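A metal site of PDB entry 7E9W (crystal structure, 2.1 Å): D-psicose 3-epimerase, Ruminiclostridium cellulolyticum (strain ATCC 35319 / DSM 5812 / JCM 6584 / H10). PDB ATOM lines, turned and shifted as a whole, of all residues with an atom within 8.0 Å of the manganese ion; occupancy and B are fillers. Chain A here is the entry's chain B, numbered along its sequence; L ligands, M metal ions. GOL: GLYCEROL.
The side-chain carboxylate (OE1) of Glu 267 sits close to a ring nitrogen (ND1) of His 232, at 3.2 Å. The guanidinium group (NH1) of Arg 238 lies close to the side-chain carboxylate (OE1) of Glu 267 (3.2 Å). N of Glu 267 is in hydrogen-bond range of O of Thr 233. The side-chain carboxylate (OD2) of Asp 206 sits close to the guanidinium group (NH1) of Arg 238, 3.9 Å away. The backbone NH (N) of Phe 208 sits at hydrogen-bond distance from the side-chain carboxylate (OD1) of Asp 206 (3.0 Å). O of Leu 205 sits at hydrogen-bond distance from N of His 232 (2.9 Å). The side-chain carboxylate (OE2) of Glu 57 lies within hydrogen-bond range of a ring nitrogen (NE2) of His 232, at 2.6 Å. The backbone carbonyl oxygen of His 232 is in hydrogen-bond range of the backbone NH of Thr 207.
Within 4 Å of the manganese ion: Glu 173, Asp 206, His 232 and Glu 267.
The manganese ion is bound by O2 of the ligand (2.0 Å), OE1 of Glu 267 (2.1 Å), OD2 of Asp 206 (2.1 Å) and OE2 of Glu 173 (2.2 Å). The manganese ion has four donor atoms within binding distance. Slightly farther from the manganese ion lies ND1 of His 232 (2.8 Å).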
ATOM      1  N   TYR A  29     -24.114 -24.277 -13.236  1.00  0.00           N
ATOM      2  CA  TYR A  29     -22.803 -24.909 -13.541  1.00  0.00           C
ATOM      3  C   TYR A  29     -22.547 -25.944 -12.443  1.00  0.00           C
ATOM      4  O   TYR A  29     -22.661 -25.587 -11.258  1.00  0.00           O
ATOM      5  CB  TYR A  29     -21.735 -23.814 -13.628  1.00  0.00           C
ATOM      6  CG  TYR A  29     -20.445 -24.173 -14.332  1.00  0.00           C
ATOM      7  CD1 TYR A  29     -20.383 -25.148 -15.321  1.00  0.00           C
ATOM      8  CD2 TYR A  29     -19.288 -23.489 -14.031  1.00  0.00           C
ATOM      9  CE1 TYR A  29     -19.196 -25.447 -15.969  1.00  0.00           C
ATOM     10  CE2 TYR A  29     -18.087 -23.775 -14.667  1.00  0.00           C
ATOM     11  CZ  TYR A  29     -18.042 -24.758 -15.643  1.00  0.00           C
ATOM     12  OH  TYR A  29     -16.860 -25.031 -16.271  1.00  0.00           O
ATOM     13  N   GLU A  57     -24.980 -27.005 -16.817  1.00  0.00           N
ATOM     14  CA  GLU A  57     -23.748 -26.660 -17.558  1.00  0.00           C
ATOM     15  C   GLU A  57     -22.617 -27.526 -17.013  1.00  0.00           C
ATOM     16  O   GLU A  57     -22.480 -27.626 -15.782  1.00  0.00           O
ATOM     17  CB  GLU A  57     -23.451 -25.160 -17.485  1.00  0.00           C
ATOM     18  CG  GLU A  57     -22.399 -24.737 -18.487  1.00  0.00           C
ATOM     19  CD  GLU A  57     -22.430 -23.257 -18.873  1.00  0.00           C
ATOM     20  OE1 GLU A  57     -23.409 -22.834 -19.571  1.00  0.00           O
ATOM     21  OE2 GLU A  57     -21.485 -22.548 -18.477  1.00  0.00           O
ATOM     22  N   GLY A 128     -19.599 -22.195 -24.477  1.00  0.00           N
ATOM     23  CA  GLY A 128     -19.237 -20.814 -24.133  1.00  0.00           C
ATOM     24  C   GLY A 128     -17.963 -20.756 -23.316  1.00  0.00           C
ATOM     25  O   GLY A 128     -17.645 -21.742 -22.643  1.00  0.00           O
ATOM     26  N   GLY A 129     -17.284 -19.614 -23.376  1.00  0.00           N
ATOM     27  CA  GLY A 129     -16.044 -19.332 -22.638  1.00  0.00           C
ATOM     28  C   GLY A 129     -15.151 -18.399 -23.417  1.00  0.00           C
ATOM     29  O   GLY A 129     -15.615 -17.824 -24.426  1.00  0.00           O
ATOM     30  N   GLU A 173     -17.320 -15.487 -24.381  1.00  0.00           N
ATOM     31  CA  GLU A 173     -17.529 -14.851 -23.046  1.00  0.00           C
ATOM     32  C   GLU A 173     -16.759 -13.537 -22.978  1.00  0.00           C
ATOM     33  O   GLU A 173     -15.542 -13.536 -23.213  1.00  0.00           O
ATOM     34  CB  GLU A 173     -17.099 -15.791 -21.917  1.00  0.00           C
ATOM     35  CG  GLU A 173     -17.451 -15.232 -20.553  1.00  0.00           C
ATOM     36  CD  GLU A 173     -17.473 -16.267 -19.440  1.00  0.00           C
ATOM     37  OE1 GLU A 173     -16.549 -17.121 -19.410  1.00  0.00           O
ATOM     38  OE2 GLU A 173     -18.432 -16.233 -18.631  1.00  0.00           O
ATOM     39  N   VAL A 174     -17.449 -12.454 -22.641  1.00  0.00           N
ATOM     40  CA  VAL A 174     -16.832 -11.142 -22.329  1.00  0.00           C
ATOM     41  C   VAL A 174     -16.339 -11.226 -20.889  1.00  0.00           C
ATOM     42  O   VAL A 174     -17.178 -11.538 -20.008  1.00  0.00           O
ATOM     43  CB  VAL A 174     -17.844 -10.001 -22.547  1.00  0.00           C
ATOM     44  CG1 VAL A 174     -17.262  -8.647 -22.188  1.00  0.00           C
ATOM     45  CG2 VAL A 174     -18.387 -10.014 -23.969  1.00  0.00           C
ATOM     46  N   LEU A 175     -15.044 -10.988 -20.654  1.00  0.00           N
ATOM     47  CA  LEU A 175     -14.360 -11.212 -19.354  1.00  0.00           C
ATOM     48  C   LEU A 175     -13.817  -9.893 -18.815  1.00  0.00           C
ATOM     49  O   LEU A 175     -13.485  -9.013 -19.622  1.00  0.00           O
ATOM     50  CB  LEU A 175     -13.205 -12.210 -19.530  1.00  0.00           C
ATOM     51  CG  LEU A 175     -13.577 -13.658 -19.835  1.00  0.00           C
ATOM     52  CD1 LEU A 175     -12.316 -14.503 -20.002  1.00  0.00           C
ATOM     53  CD2 LEU A 175     -14.454 -14.240 -18.738  1.00  0.00           C
ATOM     54  N   GLU A 179      -8.679 -11.339 -16.247  1.00  0.00           N
ATOM     55  CA  GLU A 179      -8.740 -12.728 -16.764  1.00  0.00           C
ATOM     56  C   GLU A 179      -8.438 -12.763 -18.260  1.00  0.00           C
ATOM     57  O   GLU A 179      -8.018 -13.837 -18.740  1.00  0.00           O
ATOM     58  CB  GLU A 179     -10.100 -13.334 -16.421  1.00  0.00           C
ATOM     59  CG  GLU A 179     -10.427 -13.173 -14.945  1.00  0.00           C
ATOM     60  CD  GLU A 179     -11.311 -14.252 -14.354  1.00  0.00           C
ATOM     61  OE1 GLU A 179     -10.823 -15.397 -14.222  1.00  0.00           O
ATOM     62  OE2 GLU A 179     -12.463 -13.932 -14.014  1.00  0.00           O
ATOM     63  N   MET A 204     -21.430 -13.747 -25.347  1.00  0.00           N
ATOM     64  CA  MET A 204     -21.905 -14.274 -24.050  1.00  0.00           C
ATOM     65  C   MET A 204     -21.529 -13.264 -22.959  1.00  0.00           C
ATOM     66  O   MET A 204     -20.329 -12.904 -22.864  1.00  0.00           O
ATOM     67  CB  MET A 204     -21.287 -15.640 -23.764  1.00  0.00           C
ATOM     68  CG  MET A 204     -21.573 -16.189 -22.382  1.00  0.00           C
ATOM     69  SD  MET A 204     -20.993 -17.895 -22.219  1.00  0.00           S
ATOM     70  CE  MET A 204     -20.637 -17.960 -20.470  1.00  0.00           C
ATOM     71  N   LEU A 205     -22.517 -12.817 -22.198  1.00  0.00           N
ATOM     72  CA  LEU A 205     -22.284 -11.883 -21.078  1.00  0.00           C
ATOM     73  C   LEU A 205     -22.397 -12.652 -19.758  1.00  0.00           C
ATOM     74  O   LEU A 205     -23.042 -13.722 -19.722  1.00  0.00           O
ATOM     75  CB  LEU A 205     -23.291 -10.734 -21.147  1.00  0.00           C
ATOM     76  CG  LEU A 205     -23.199  -9.869 -22.402  1.00  0.00           C
ATOM     77  CD1 LEU A 205     -24.263  -8.779 -22.393  1.00  0.00           C
ATOM     78  CD2 LEU A 205     -21.804  -9.256 -22.547  1.00  0.00           C
ATOM     79  N   ASP A 206     -21.738 -12.103 -18.737  1.00  0.00           N
ATOM     80  CA  ASP A 206     -21.655 -12.656 -17.362  1.00  0.00           C
ATOM     81  C   ASP A 206     -21.780 -11.481 -16.394  1.00  0.00           C
ATOM     82  O   ASP A 206     -20.986 -10.539 -16.503  1.00  0.00           O
ATOM     83  CB  ASP A 206     -20.338 -13.405 -17.175  1.00  0.00           C
ATOM     84  CG  ASP A 206     -20.262 -14.199 -15.890  1.00  0.00           C
ATOM     85  OD1 ASP A 206     -20.731 -13.699 -14.848  1.00  0.00           O
ATOM     86  OD2 ASP A 206     -19.731 -15.318 -15.940  1.00  0.00           O
ATOM     87  N   THR A 207     -22.766 -11.546 -15.485  1.00  0.00           N
ATOM     88  CA  THR A 207     -23.085 -10.470 -14.513  1.00  0.00           C
ATOM     89  C   THR A 207     -21.844 -10.167 -13.682  1.00  0.00           C
ATOM     90  O   THR A 207     -21.626  -8.985 -13.386  1.00  0.00           O
ATOM     91  CB  THR A 207     -24.311 -10.855 -13.688  1.00  0.00           C
ATOM     92  OG1 THR A 207     -24.011 -12.070 -12.988  1.00  0.00           O
ATOM     93  CG2 THR A 207     -25.542 -11.050 -14.552  1.00  0.00           C
ATOM     94  N   PHE A 208     -21.050 -11.185 -13.332  1.00  0.00           N
ATOM     95  CA  PHE A 208     -19.791 -11.016 -12.548  1.00  0.00           C
ATOM     96  C   PHE A 208     -18.816 -10.119 -13.335  1.00  0.00           C
ATOM     97  O   PHE A 208     -18.171  -9.225 -12.729  1.00  0.00           O
ATOM     98  CB  PHE A 208     -19.162 -12.370 -12.205  1.00  0.00           C
ATOM     99  CG  PHE A 208     -17.808 -12.276 -11.558  1.00  0.00           C
ATOM    100  CD1 PHE A 208     -17.656 -11.789 -10.270  1.00  0.00           C
ATOM    101  CD2 PHE A 208     -16.663 -12.642 -12.254  1.00  0.00           C
ATOM    102  CE1 PHE A 208     -16.411 -11.697  -9.678  1.00  0.00           C
ATOM    103  CE2 PHE A 208     -15.413 -12.546 -11.671  1.00  0.00           C
ATOM    104  CZ  PHE A 208     -15.282 -12.067 -10.384  1.00  0.00           C
ATOM    105  N   HIS A 209     -18.689 -10.355 -14.644  1.00  0.00           N
ATOM    106  CA  HIS A 209     -17.713  -9.662 -15.526  1.00  0.00           C
ATOM    107  C   HIS A 209     -18.243  -8.263 -15.873  1.00  0.00           C
ATOM    108  O   HIS A 209     -17.463  -7.308 -15.781  1.00  0.00           O
ATOM    109  CB  HIS A 209     -17.392 -10.528 -16.734  1.00  0.00           C
ATOM    110  CG  HIS A 209     -16.631 -11.759 -16.357  1.00  0.00           C
ATOM    111  ND1 HIS A 209     -15.422 -11.685 -15.696  1.00  0.00           N
ATOM    112  CD2 HIS A 209     -16.910 -13.062 -16.507  1.00  0.00           C
ATOM    113  CE1 HIS A 209     -14.993 -12.915 -15.474  1.00  0.00           C
ATOM    114  NE2 HIS A 209     -15.886 -13.772 -15.951  1.00  0.00           N
ATOM    115  N   HIS A 230     -25.935 -16.352 -24.874  1.00  0.00           N
ATOM    116  CA  HIS A 230     -25.898 -17.018 -23.544  1.00  0.00           C
ATOM    117  C   HIS A 230     -25.630 -15.978 -22.459  1.00  0.00           C
ATOM    118  O   HIS A 230     -24.899 -14.993 -22.737  1.00  0.00           O
ATOM    119  CB  HIS A 230     -24.849 -18.139 -23.538  1.00  0.00           C
ATOM    120  CG  HIS A 230     -25.084 -19.183 -22.500  1.00  0.00           C
ATOM    121  ND1 HIS A 230     -26.336 -19.677 -22.198  1.00  0.00           N
ATOM    122  CD2 HIS A 230     -24.218 -19.864 -21.701  1.00  0.00           C
ATOM    123  CE1 HIS A 230     -26.236 -20.585 -21.258  1.00  0.00           C
ATOM    124  NE2 HIS A 230     -24.952 -20.729 -20.935  1.00  0.00           N
ATOM    125  N   LEU A 231     -26.204 -16.185 -21.282  1.00  0.00           N
ATOM    126  CA  LEU A 231     -26.041 -15.311 -20.103  1.00  0.00           C
ATOM    127  C   LEU A 231     -25.640 -16.161 -18.892  1.00  0.00           C
ATOM    128  O   LEU A 231     -26.403 -17.081 -18.521  1.00  0.00           O
ATOM    129  CB  LEU A 231     -27.334 -14.533 -19.837  1.00  0.00           C
ATOM    130  CG  LEU A 231     -27.275 -13.554 -18.655  1.00  0.00           C
ATOM    131  CD1 LEU A 231     -26.302 -12.411 -18.937  1.00  0.00           C
ATOM    132  CD2 LEU A 231     -28.648 -13.011 -18.334  1.00  0.00           C
ATOM    133  N   HIS A 232     -24.496 -15.854 -18.300  1.00  0.00           N
ATOM    134  CA  HIS A 232     -24.053 -16.361 -16.975  1.00  0.00           C
ATOM    135  C   HIS A 232     -24.464 -15.374 -15.895  1.00  0.00           C
ATOM    136  O   HIS A 232     -24.390 -14.156 -16.131  1.00  0.00           O
ATOM    137  CB  HIS A 232     -22.553 -16.669 -16.969  1.00  0.00           C
ATOM    138  CG  HIS A 232     -22.244 -18.009 -17.531  1.00  0.00           C
ATOM    139  ND1 HIS A 232     -20.957 -18.473 -17.671  1.00  0.00           N
ATOM    140  CD2 HIS A 232     -23.047 -19.001 -17.995  1.00  0.00           C
ATOM    141  CE1 HIS A 232     -20.975 -19.688 -18.179  1.00  0.00           C
ATOM    142  NE2 HIS A 232     -22.239 -20.024 -18.415  1.00  0.00           N
ATOM    143  N   THR A 233     -24.894 -15.896 -14.739  1.00  0.00           N
ATOM    144  CA  THR A 233     -25.355 -15.094 -13.592  1.00  0.00           C
ATOM    145  C   THR A 233     -24.574 -15.491 -12.339  1.00  0.00           C
ATOM    146  O   THR A 233     -24.096 -16.645 -12.228  1.00  0.00           O
ATOM    147  CB  THR A 233     -26.875 -15.203 -13.423  1.00  0.00           C
ATOM    148  OG1 THR A 233     -27.203 -16.586 -13.261  1.00  0.00           O
ATOM    149  CG2 THR A 233     -27.641 -14.606 -14.587  1.00  0.00           C
ATOM    150  N   ARG A 238     -19.704 -13.623  -6.699  1.00  0.00           N
ATOM    151  CA  ARG A 238     -19.994 -14.949  -7.305  1.00  0.00           C
ATOM    152  C   ARG A 238     -20.869 -15.796  -6.364  1.00  0.00           C
ATOM    153  O   ARG A 238     -20.921 -17.032  -6.564  1.00  0.00           O
ATOM    154  CB  ARG A 238     -18.701 -15.693  -7.665  1.00  0.00           C
ATOM    155  CG  ARG A 238     -17.655 -14.820  -8.343  1.00  0.00           C
ATOM    156  CD  ARG A 238     -16.791 -15.579  -9.330  1.00  0.00           C
ATOM    157  NE  ARG A 238     -17.504 -15.824 -10.563  1.00  0.00           N
ATOM    158  CZ  ARG A 238     -16.930 -16.105 -11.737  1.00  0.00           C
ATOM    159  NH1 ARG A 238     -17.677 -16.327 -12.798  1.00  0.00           N
ATOM    160  NH2 ARG A 238     -15.608 -16.156 -11.833  1.00  0.00           N
ATOM    161  N   VAL A 265     -27.832 -19.306 -17.172  1.00  0.00           N
ATOM    162  CA  VAL A 265     -27.110 -20.321 -16.356  1.00  0.00           C
ATOM    163  C   VAL A 265     -26.368 -19.596 -15.234  1.00  0.00           C
ATOM    164  O   VAL A 265     -25.501 -18.761 -15.553  1.00  0.00           O
ATOM    165  CB  VAL A 265     -26.165 -21.154 -17.237  1.00  0.00           C
ATOM    166  CG1 VAL A 265     -25.134 -21.915 -16.413  1.00  0.00           C
ATOM    167  CG2 VAL A 265     -26.935 -22.106 -18.133  1.00  0.00           C
ATOM    168  N   MET A 266     -26.710 -19.883 -13.986  1.00  0.00           N
ATOM    169  CA  MET A 266     -25.999 -19.307 -12.821  1.00  0.00           C
ATOM    170  C   MET A 266     -24.674 -20.062 -12.645  1.00  0.00           C
ATOM    171  O   MET A 266     -24.639 -21.282 -12.878  1.00  0.00           O
ATOM    172  CB  MET A 266     -26.814 -19.300 -11.523  1.00  0.00           C
ATOM    173  CG  MET A 266     -27.388 -20.631 -11.117  1.00  0.00           C
ATOM    174  SD  MET A 266     -28.404 -20.466  -9.629  1.00  0.00           S
ATOM    175  CE  MET A 266     -29.814 -19.574 -10.268  1.00  0.00           C
ATOM    176  N   GLU A 267     -23.641 -19.329 -12.267  1.00  0.00           N
ATOM    177  CA  GLU A 267     -22.237 -19.792 -12.205  1.00  0.00           C
ATOM    178  C   GLU A 267     -21.680 -19.382 -10.840  1.00  0.00           C
ATOM    179  O   GLU A 267     -20.692 -18.645 -10.769  1.00  0.00           O
ATOM    180  CB  GLU A 267     -21.491 -19.178 -13.391  1.00  0.00           C
ATOM    181  CG  GLU A 267     -20.343 -20.019 -13.911  1.00  0.00           C
ATOM    182  CD  GLU A 267     -19.396 -19.282 -14.838  1.00  0.00           C
ATOM    183  OE1 GLU A 267     -19.447 -18.019 -14.893  1.00  0.00           O
ATOM    184  OE2 GLU A 267     -18.594 -19.966 -15.502  1.00  0.00           O
ATOM    185  N   PHE A 269     -19.715 -19.548  -7.325  1.00  0.00           N
ATOM    186  CA  PHE A 269     -18.478 -20.148  -6.748  1.00  0.00           C
ATOM    187  C   PHE A 269     -18.329 -19.607  -5.331  1.00  0.00           C
ATOM    188  O   PHE A 269     -18.075 -18.386  -5.191  1.00  0.00           O
ATOM    189  CB  PHE A 269     -17.261 -19.802  -7.605  1.00  0.00           C
ATOM    190  CG  PHE A 269     -17.249 -20.385  -8.982  1.00  0.00           C
ATOM    191  CD1 PHE A 269     -16.930 -21.723  -9.180  1.00  0.00           C
ATOM    192  CD2 PHE A 269     -17.497 -19.594 -10.092  1.00  0.00           C
ATOM    193  CE1 PHE A 269     -16.889 -22.255 -10.463  1.00  0.00           C
ATOM    194  CE2 PHE A 269     -17.457 -20.138 -11.368  1.00  0.00           C
ATOM    195  CZ  PHE A 269     -17.148 -21.462 -11.554  1.00  0.00           C
ATOM    196  N   ILE A 280     -10.722 -19.681  -9.566  1.00  0.00           N
ATOM    197  CA  ILE A 280     -11.799 -18.679  -9.302  1.00  0.00           C
ATOM    198  C   ILE A 280     -11.342 -17.722  -8.191  1.00  0.00           C
ATOM    199  O   ILE A 280     -12.000 -16.675  -8.020  1.00  0.00           O
ATOM    200  CB  ILE A 280     -13.148 -19.364  -8.972  1.00  0.00           C
ATOM    201  CG1 ILE A 280     -13.561 -20.342 -10.070  1.00  0.00           C
ATOM    202  CG2 ILE A 280     -14.235 -18.334  -8.702  1.00  0.00           C
ATOM    203  CD1 ILE A 280     -13.647 -19.732 -11.459  1.00  0.00           C
HETATM  204  C1  GOL L   1     -15.579 -18.691 -14.921  1.00  0.00           C
HETATM  205  O1  GOL L   1     -15.884 -19.974 -15.457  1.00  0.00           O
HETATM  206  C2  GOL L   1     -15.584 -17.613 -15.982  1.00  0.00           C
HETATM  207  O2  GOL L   1     -16.877 -16.982 -16.050  1.00  0.00           O
HETATM  208  C3  GOL L   1     -14.474 -16.587 -15.815  1.00  0.00           C
HETATM  209  O3  GOL L   1     -14.190 -16.280 -14.450  1.00  0.00           O
HETATM  210 MN    MN M   1     -18.775 -17.077 -16.648  1.00  0.00          MN
